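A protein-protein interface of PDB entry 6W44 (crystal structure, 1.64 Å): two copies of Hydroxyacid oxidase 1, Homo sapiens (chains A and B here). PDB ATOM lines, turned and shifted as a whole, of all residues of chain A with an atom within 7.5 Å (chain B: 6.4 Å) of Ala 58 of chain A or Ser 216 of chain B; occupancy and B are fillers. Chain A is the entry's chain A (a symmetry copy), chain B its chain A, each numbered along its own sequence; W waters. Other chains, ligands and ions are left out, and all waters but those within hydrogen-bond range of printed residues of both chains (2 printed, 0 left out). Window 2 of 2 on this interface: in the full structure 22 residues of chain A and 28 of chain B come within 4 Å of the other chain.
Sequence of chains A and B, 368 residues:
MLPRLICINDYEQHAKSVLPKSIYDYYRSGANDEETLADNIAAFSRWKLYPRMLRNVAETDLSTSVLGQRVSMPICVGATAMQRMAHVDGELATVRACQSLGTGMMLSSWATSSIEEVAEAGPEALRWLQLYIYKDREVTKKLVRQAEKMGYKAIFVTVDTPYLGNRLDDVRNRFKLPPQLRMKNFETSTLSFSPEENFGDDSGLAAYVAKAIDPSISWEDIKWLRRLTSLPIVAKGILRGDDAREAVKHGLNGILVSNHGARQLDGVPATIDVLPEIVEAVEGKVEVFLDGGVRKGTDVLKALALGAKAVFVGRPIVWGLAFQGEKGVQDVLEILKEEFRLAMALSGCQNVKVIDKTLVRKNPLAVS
Water W2 lies within hydrogen-bond range of the backbone carbonyl oxygen (O) of Ile 217 of chain B (2.7 Å), the backbone carbonyl oxygen (O) of Pro 215 of chain B (2.8 Å) and the backbone NH (N) of Asn 56 of chain A (3.3 Å). Water W1 bridges the side-chain hydroxyl (OG1) of Thr 60 of chain A (2.7 Å) and the side-chain hydroxyl (OH) of Tyr 163 of chain B (2.8 Å).
The backbone carbonyl oxygen of Val 57 of chain A sits at hydrogen-bond distance from the side-chain hydroxyl of Tyr 163 of chain B (3.2 Å). OH of Tyr 163 of chain B is in hydrogen-bond range of O of Ala 58 of chain A (3.5 Å). The backbone NH (N) of Val 57 of chain A is in hydrogen-bond range of the backbone carbonyl oxygen (O) of Pro 215 of chain B (3.1 Å). The backbone NH (N) of Ala 58 of chain A lies within hydrogen-bond range of the backbone carbonyl oxygen (O) of Pro 215 of chain B, 3.5 Å away. The backbone NH (N) of Asn 56 of chain A lies within hydrogen-bond range of the backbone carbonyl oxygen (O) of Ile 217 of chain B (3.4 Å).
Of the 10 printed residues of chain B, 6 touch a printed residue of chain A. Of the 11 printed residues of chain A, 6 touch a printed residue of chain B. Printed residues of chain A that touch a printed residue of chain B: Leu 54, Arg 55, Asn 56, Val 57, Ala 58 and Ala 345. Among the printed residues, 14 pairs touch across the chains. Among the printed residues, no Asp or Glu carboxylate lies within 4 Å of a Lys or Arg side-chain nitrogen of the other chain.
The side-chain hydroxyl of Ser 216 of chain B lies within hydrogen-bond range of the side-chain carboxylate of Asp 214 of chain B, at 2.6 Å. OD2 of Asp 221 of chain B is in hydrogen-bond range of N of Ser 218 of chain B (2.9 Å). NE2 of Gln 350 of chain A sits at hydrogen-bond distance from O of Arg 55 of chain A (2.5 Å). The backbone NH (N) of Ala 58 of chain A is in hydrogen-bond range of the side-chain amide oxygen (OD1) of Asn 56 of chain A, 3.2 Å away. NE2 of Gln 350 of chain A sits close to O of Asn 56 of chain A, 3.2 Å away.
CD1 of Ile 217 of chain B touches CD2 of Leu 54 of chain A, at 3.3 Å. Ser 218 of chain B touches Leu 54 of chain A. Arg 55 of chain A touches Ile 217 of chain B (N to O, 3.8 Å). Asn 56 of chain A touches Pro 215 of chain B. Ser 216 of chain B touches Asn 56 of chain A. Val 57 of chain A touches Pro 162 of chain B. CB of Ser 216 of chain B touches CB of Ala 58 of chain A, at 3.9 Å. Ala 345 of chain A touches Pro 162 of chain B. CB of Ala 345 of chain A touches CE2 of Tyr 163 of chain B, at 3.7 Å.
No position is printed for both chains. Of the 14 pairs that touch across the chains among the printed residues, none has its exchanged pair printed and touching as well.
Ala 58 of chain A touches just these residues of chain B: Tyr 163 (3.5 Å), Pro 215 (3.5 Å) and Ser 216 (3.9 Å). Printed residues of chain A within 4 Å of Ser 216 of chain B: Asn 56 and Ala 58. Of the printed residues of chain A, Ser 218 of chain B touches Leu 54 (3.3 Å). Printed residues of chain B within 4 Å of Arg 55 of chain A: Ile 217. Of the printed residues of chain A, Tyr 163 of chain B touches Val 57 (3.2 Å), Ala 58 (3.5 Å) and Ala 345 (3.7 Å). Arg 341 of chain A touches none of the printed residues of chain B. The nearest residue of chain B that does not touch Ala 58 of chain A is Asp 214 of chain B (5.5 Å). The nearest residue of chain A that does not touch Ser 216 of chain B is Val 57 of chain A (4.5 Å). The nearest printed residue of chain A that does not touch Ile 217 of chain B is Val 57 of chain A (5.3 Å).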
ATOM      1  N   LEU A  54      -4.879  20.244  14.554  1.00  0.00           N
ATOM      2  CA  LEU A  54      -4.021  21.014  15.513  1.00  0.00           C
ATOM      3  C   LEU A  54      -2.590  20.486  15.476  1.00  0.00           C
ATOM      4  O   LEU A  54      -1.941  20.350  16.573  1.00  0.00           O
ATOM      5  CB  LEU A  54      -4.631  20.953  16.914  1.00  0.00           C
ATOM      6  CG  LEU A  54      -6.034  21.548  16.977  1.00  0.00           C
ATOM      7  CD1 LEU A  54      -6.729  21.213  18.296  1.00  0.00           C
ATOM      8  CD2 LEU A  54      -6.006  23.023  16.737  1.00  0.00           C
ATOM      9  N   ARG A  55      -2.071  20.221  14.275  1.00  0.00           N
ATOM     10  CA  ARG A  55      -0.688  19.685  14.172  1.00  0.00           C
ATOM     11  C   ARG A  55       0.344  20.740  13.764  1.00  0.00           C
ATOM     12  O   ARG A  55       1.536  20.387  13.766  1.00  0.00           O
ATOM     13  CB  ARG A  55      -0.595  18.519  13.198  1.00  0.00           C
ATOM     14  CG  ARG A  55      -1.609  17.401  13.418  1.00  0.00           C
ATOM     15  CD  ARG A  55      -1.627  16.873  14.804  1.00  0.00           C
ATOM     16  NE  ARG A  55      -0.396  16.218  15.142  1.00  0.00           N
ATOM     17  CZ  ARG A  55      -0.198  15.554  16.281  1.00  0.00           C
ATOM     18  NH1 ARG A  55       0.976  14.988  16.517  1.00  0.00           N
ATOM     19  NH2 ARG A  55      -1.151  15.478  17.198  1.00  0.00           N
ATOM     20  N   ASN A  56      -0.057  21.918  13.314  1.00  0.00           N
ATOM     21  CA  ASN A  56       0.811  22.993  12.760  1.00  0.00           C
ATOM     22  C   ASN A  56       1.245  22.635  11.337  1.00  0.00           C
ATOM     23  O   ASN A  56       2.263  21.943  11.132  1.00  0.00           O
ATOM     24  CB  ASN A  56       2.056  23.347  13.574  1.00  0.00           C
ATOM     25  CG  ASN A  56       2.807  24.496  12.963  1.00  0.00           C
ATOM     26  OD1 ASN A  56       2.501  25.007  11.872  1.00  0.00           O
ATOM     27  ND2 ASN A  56       3.764  25.005  13.725  1.00  0.00           N
ATOM     28  N   VAL A  57       0.448  23.072  10.372  1.00  0.00           N
ATOM     29  CA  VAL A  57       0.677  22.759   8.933  1.00  0.00           C
ATOM     30  C   VAL A  57       0.951  24.048   8.171  1.00  0.00           C
ATOM     31  O   VAL A  57       0.714  24.084   6.947  1.00  0.00           O
ATOM     32  CB  VAL A  57      -0.530  21.983   8.376  1.00  0.00           C
ATOM     33  CG1 VAL A  57      -0.535  20.572   8.925  1.00  0.00           C
ATOM     34  CG2 VAL A  57      -1.851  22.682   8.667  1.00  0.00           C
ATOM     35  N   ALA A  58       1.522  25.054   8.835  1.00  0.00           N
ATOM     36  CA  ALA A  58       1.902  26.302   8.164  1.00  0.00           C
ATOM     37  C   ALA A  58       2.928  26.038   7.067  1.00  0.00           C
ATOM     38  O   ALA A  58       2.927  26.810   6.043  1.00  0.00           O
ATOM     39  CB  ALA A  58       2.468  27.270   9.171  1.00  0.00           C
ATOM     40  N   GLU A  59       3.820  25.086   7.237  1.00  0.00           N
ATOM     41  CA  GLU A  59       4.884  25.029   6.188  1.00  0.00           C
ATOM     42  C   GLU A  59       4.955  23.682   5.483  1.00  0.00           C
ATOM     43  O   GLU A  59       5.950  22.954   5.674  1.00  0.00           O
ATOM     44  CB  GLU A  59       6.258  25.293   6.782  1.00  0.00           C
ATOM     45  CG  GLU A  59       6.474  26.738   7.129  1.00  0.00           C
ATOM     46  CD  GLU A  59       7.444  26.824   8.287  1.00  0.00           C
ATOM     47  OE1 GLU A  59       7.017  26.524   9.426  1.00  0.00           O
ATOM     48  OE2 GLU A  59       8.629  27.129   8.045  1.00  0.00           O
ATOM     49  N   THR A  60       3.975  23.374   4.674  1.00  0.00           N
ATOM     50  CA  THR A  60       3.858  21.986   4.151  1.00  0.00           C
ATOM     51  C   THR A  60       4.973  21.763   3.134  1.00  0.00           C
ATOM     52  O   THR A  60       5.379  22.718   2.423  1.00  0.00           O
ATOM     53  CB  THR A  60       2.470  21.779   3.592  1.00  0.00           C
ATOM     54  OG1 THR A  60       2.474  22.828   2.617  1.00  0.00           O
ATOM     55  CG2 THR A  60       1.441  21.885   4.690  1.00  0.00           C
ATOM     56  N   ASP A  61       5.592  20.597   3.222  1.00  0.00           N
ATOM     57  CA  ASP A  61       6.736  20.217   2.384  1.00  0.00           C
ATOM     58  C   ASP A  61       6.324  18.935   1.667  1.00  0.00           C
ATOM     59  O   ASP A  61       6.110  17.897   2.356  1.00  0.00           O
ATOM     60  CB  ASP A  61       7.973  19.992   3.226  1.00  0.00           C
ATOM     61  CG  ASP A  61       9.218  19.574   2.483  1.00  0.00           C
ATOM     62  OD1 ASP A  61       9.146  19.261   1.282  1.00  0.00           O
ATOM     63  OD2 ASP A  61      10.272  19.509   3.141  1.00  0.00           O
ATOM     64  N   ARG A 341      -1.250  19.273  -1.499  1.00  0.00           N
ATOM     65  CA  ARG A 341      -0.817  20.149  -0.372  1.00  0.00           C
ATOM     66  C   ARG A 341      -2.001  20.389   0.555  1.00  0.00           C
ATOM     67  O   ARG A 341      -1.872  20.304   1.791  1.00  0.00           O
ATOM     68  CB  ARG A 341      -0.252  21.474  -0.878  1.00  0.00           C
ATOM     69  CG  ARG A 341       0.361  22.292   0.240  1.00  0.00           C
ATOM     70  CD  ARG A 341       0.772  23.668  -0.235  1.00  0.00           C
ATOM     71  NE  ARG A 341       1.623  23.634  -1.414  1.00  0.00           N
ATOM     72  CZ  ARG A 341       2.929  23.389  -1.479  1.00  0.00           C
ATOM     73  NH1 ARG A 341       3.653  23.072  -0.414  1.00  0.00           N
ATOM     74  NH2 ARG A 341       3.516  23.451  -2.663  1.00  0.00           N
ATOM     75  N   ALA A 345      -2.387  19.249   4.472  1.00  0.00           N
ATOM     76  CA  ALA A 345      -2.568  20.261   5.531  1.00  0.00           C
ATOM     77  C   ALA A 345      -3.855  19.943   6.317  1.00  0.00           C
ATOM     78  O   ALA A 345      -3.833  19.969   7.559  1.00  0.00           O
ATOM     79  CB  ALA A 345      -2.572  21.628   4.908  1.00  0.00           C
ATOM     80  N   GLN A 350       2.530  17.698   7.895  1.00  0.00           N
ATOM     81  CA  GLN A 350       3.471  18.788   7.540  1.00  0.00           C
ATOM     82  C   GLN A 350       4.320  18.367   6.350  1.00  0.00           C
ATOM     83  O   GLN A 350       4.725  19.244   5.557  1.00  0.00           O
ATOM     84  CB  GLN A 350       4.385  19.070   8.733  1.00  0.00           C
ATOM     85  CG  GLN A 350       3.599  19.573   9.929  1.00  0.00           C
ATOM     86  CD  GLN A 350       3.129  18.532  10.918  1.00  0.00           C
ATOM     87  OE1 GLN A 350       2.924  17.331  10.632  1.00  0.00           O
ATOM     88  NE2 GLN A 350       2.920  19.026  12.132  1.00  0.00           N
ATOM     89  N   ARG B 137      -3.681  37.340  17.326  1.00  0.00           N
ATOM     90  CA  ARG B 137      -4.159  36.827  18.619  1.00  0.00           C
ATOM     91  C   ARG B 137      -4.811  37.977  19.393  1.00  0.00           C
ATOM     92  O   ARG B 137      -5.632  37.689  20.264  1.00  0.00           O
ATOM     93  CB  ARG B 137      -3.028  36.163  19.399  1.00  0.00           C
ATOM     94  CG  ARG B 137      -2.414  34.958  18.721  1.00  0.00           C
ATOM     95  CD  ARG B 137      -3.368  33.756  18.672  1.00  0.00           C
ATOM     96  NE  ARG B 137      -2.607  32.545  18.463  1.00  0.00           N
ATOM     97  CZ  ARG B 137      -2.151  32.155  17.273  1.00  0.00           C
ATOM     98  NH1 ARG B 137      -2.474  32.831  16.192  1.00  0.00           N
ATOM     99  NH2 ARG B 137      -1.411  31.071  17.185  1.00  0.00           N
ATOM    100  N   PRO B 162      -7.276  24.856   9.168  1.00  0.00           N
ATOM    101  CA  PRO B 162      -5.977  25.524   9.069  1.00  0.00           C
ATOM    102  C   PRO B 162      -5.979  26.373   7.785  1.00  0.00           C
ATOM    103  O   PRO B 162      -5.374  27.362   7.768  1.00  0.00           O
ATOM    104  CB  PRO B 162      -4.966  24.378   8.993  1.00  0.00           C
ATOM    105  CG  PRO B 162      -5.784  23.172   8.588  1.00  0.00           C
ATOM    106  CD  PRO B 162      -7.154  23.417   9.174  1.00  0.00           C
ATOM    107  N   TYR B 163      -6.600  25.844   6.739  1.00  0.00           N
ATOM    108  CA  TYR B 163      -6.892  26.502   5.451  1.00  0.00           C
ATOM    109  C   TYR B 163      -8.360  26.212   5.111  1.00  0.00           C
ATOM    110  O   TYR B 163      -8.915  25.285   5.611  1.00  0.00           O
ATOM    111  CB  TYR B 163      -5.992  25.932   4.355  1.00  0.00           C
ATOM    112  CG  TYR B 163      -4.514  26.113   4.573  1.00  0.00           C
ATOM    113  CD1 TYR B 163      -3.869  27.272   4.198  1.00  0.00           C
ATOM    114  CD2 TYR B 163      -3.764  25.132   5.178  1.00  0.00           C
ATOM    115  CE1 TYR B 163      -2.514  27.433   4.412  1.00  0.00           C
ATOM    116  CE2 TYR B 163      -2.408  25.265   5.377  1.00  0.00           C
ATOM    117  CZ  TYR B 163      -1.776  26.427   4.996  1.00  0.00           C
ATOM    118  OH  TYR B 163      -0.448  26.560   5.227  1.00  0.00           O
ATOM    119  N   ILE B 213      -6.904  33.491   8.903  1.00  0.00           N
ATOM    120  CA  ILE B 213      -6.857  32.222   9.687  1.00  0.00           C
ATOM    121  C   ILE B 213      -5.427  31.678   9.724  1.00  0.00           C
ATOM    122  O   ILE B 213      -4.742  31.624   8.685  1.00  0.00           O
ATOM    123  CB  ILE B 213      -7.811  31.162   9.086  1.00  0.00           C
ATOM    124  CG1 ILE B 213      -9.252  31.644   8.954  1.00  0.00           C
ATOM    125  CG2 ILE B 213      -7.716  29.875   9.880  1.00  0.00           C
ATOM    126  CD1 ILE B 213      -9.825  32.190  10.198  1.00  0.00           C
ATOM    127  N   ASP B 214      -5.015  31.217  10.895  1.00  0.00           N
ATOM    128  CA  ASP B 214      -3.641  30.753  11.164  1.00  0.00           C
ATOM    129  C   ASP B 214      -3.519  29.246  10.896  1.00  0.00           C
ATOM    130  O   ASP B 214      -4.114  28.453  11.623  1.00  0.00           O
ATOM    131  CB  ASP B 214      -3.281  31.096  12.603  1.00  0.00           C
ATOM    132  CG  ASP B 214      -1.804  30.946  12.918  1.00  0.00           C
ATOM    133  OD1 ASP B 214      -1.091  30.260  12.163  1.00  0.00           O
ATOM    134  OD2 ASP B 214      -1.393  31.512  13.957  1.00  0.00           O
ATOM    135  N   PRO B 215      -2.744  28.813   9.880  1.00  0.00           N
ATOM    136  CA  PRO B 215      -2.487  27.392   9.637  1.00  0.00           C
ATOM    137  C   PRO B 215      -1.540  26.724  10.633  1.00  0.00           C
ATOM    138  O   PRO B 215      -1.404  25.538  10.610  1.00  0.00           O
ATOM    139  CB  PRO B 215      -1.895  27.383   8.225  1.00  0.00           C
ATOM    140  CG  PRO B 215      -1.206  28.733   8.102  1.00  0.00           C
ATOM    141  CD  PRO B 215      -2.089  29.684   8.886  1.00  0.00           C
ATOM    142  N   SER B 216      -0.876  27.516  11.484  1.00  0.00           N
ATOM    143  CA  SER B 216       0.076  26.978  12.475  1.00  0.00           C
ATOM    144  C   SER B 216      -0.596  26.516  13.767  1.00  0.00           C
ATOM    145  O   SER B 216       0.120  25.966  14.609  1.00  0.00           O
ATOM    146  CB  SER B 216       1.177  27.980  12.788  1.00  0.00           C
ATOM    147  OG  SER B 216       0.661  29.011  13.599  1.00  0.00           O
ATOM    148  N   ILE B 217      -1.915  26.663  13.902  1.00  0.00           N
ATOM    149  CA  ILE B 217      -2.677  26.377  15.153  1.00  0.00           C
ATOM    150  C   ILE B 217      -2.336  24.952  15.636  1.00  0.00           C
ATOM    151  O   ILE B 217      -2.359  23.989  14.823  1.00  0.00           O
ATOM    152  CB  ILE B 217      -4.177  26.637  14.879  1.00  0.00           C
ATOM    153  CG1 ILE B 217      -5.088  26.383  16.075  1.00  0.00           C
ATOM    154  CG2 ILE B 217      -4.654  25.851  13.687  1.00  0.00           C
ATOM    155  CD1 ILE B 217      -6.511  26.137  15.653  1.00  0.00           C
ATOM    156  N   SER B 218      -1.916  24.810  16.889  1.00  0.00           N
ATOM    157  CA  SER B 218      -1.552  23.514  17.488  1.00  0.00           C
ATOM    158  C   SER B 218      -2.241  23.365  18.834  1.00  0.00           C
ATOM    159  O   SER B 218      -2.959  24.290  19.285  1.00  0.00           O
ATOM    160  CB  SER B 218      -0.050  23.403  17.636  1.00  0.00           C
ATOM    161  OG  SER B 218       0.364  24.190  18.743  1.00  0.00           O
ATOM    162  N   ASP B 221      -1.833  26.205  21.189  1.00  0.00           N
ATOM    163  CA  ASP B 221      -2.783  27.330  21.060  1.00  0.00           C
ATOM    164  C   ASP B 221      -4.091  27.019  21.820  1.00  0.00           C
ATOM    165  O   ASP B 221      -4.738  27.951  22.318  1.00  0.00           O
ATOM    166  CB  ASP B 221      -3.014  27.684  19.598  1.00  0.00           C
ATOM    167  CG  ASP B 221      -1.706  28.085  18.953  1.00  0.00           C
ATOM    168  OD1 ASP B 221      -1.118  29.108  19.407  1.00  0.00           O
ATOM    169  OD2 ASP B 221      -1.217  27.354  18.095  1.00  0.00           O
HETATM  170  O   HOH W   1       1.136  24.994   3.547  1.00  0.00           O
HETATM  171  O   HOH W   2      -2.653  23.570  12.212  1.00  0.00           O
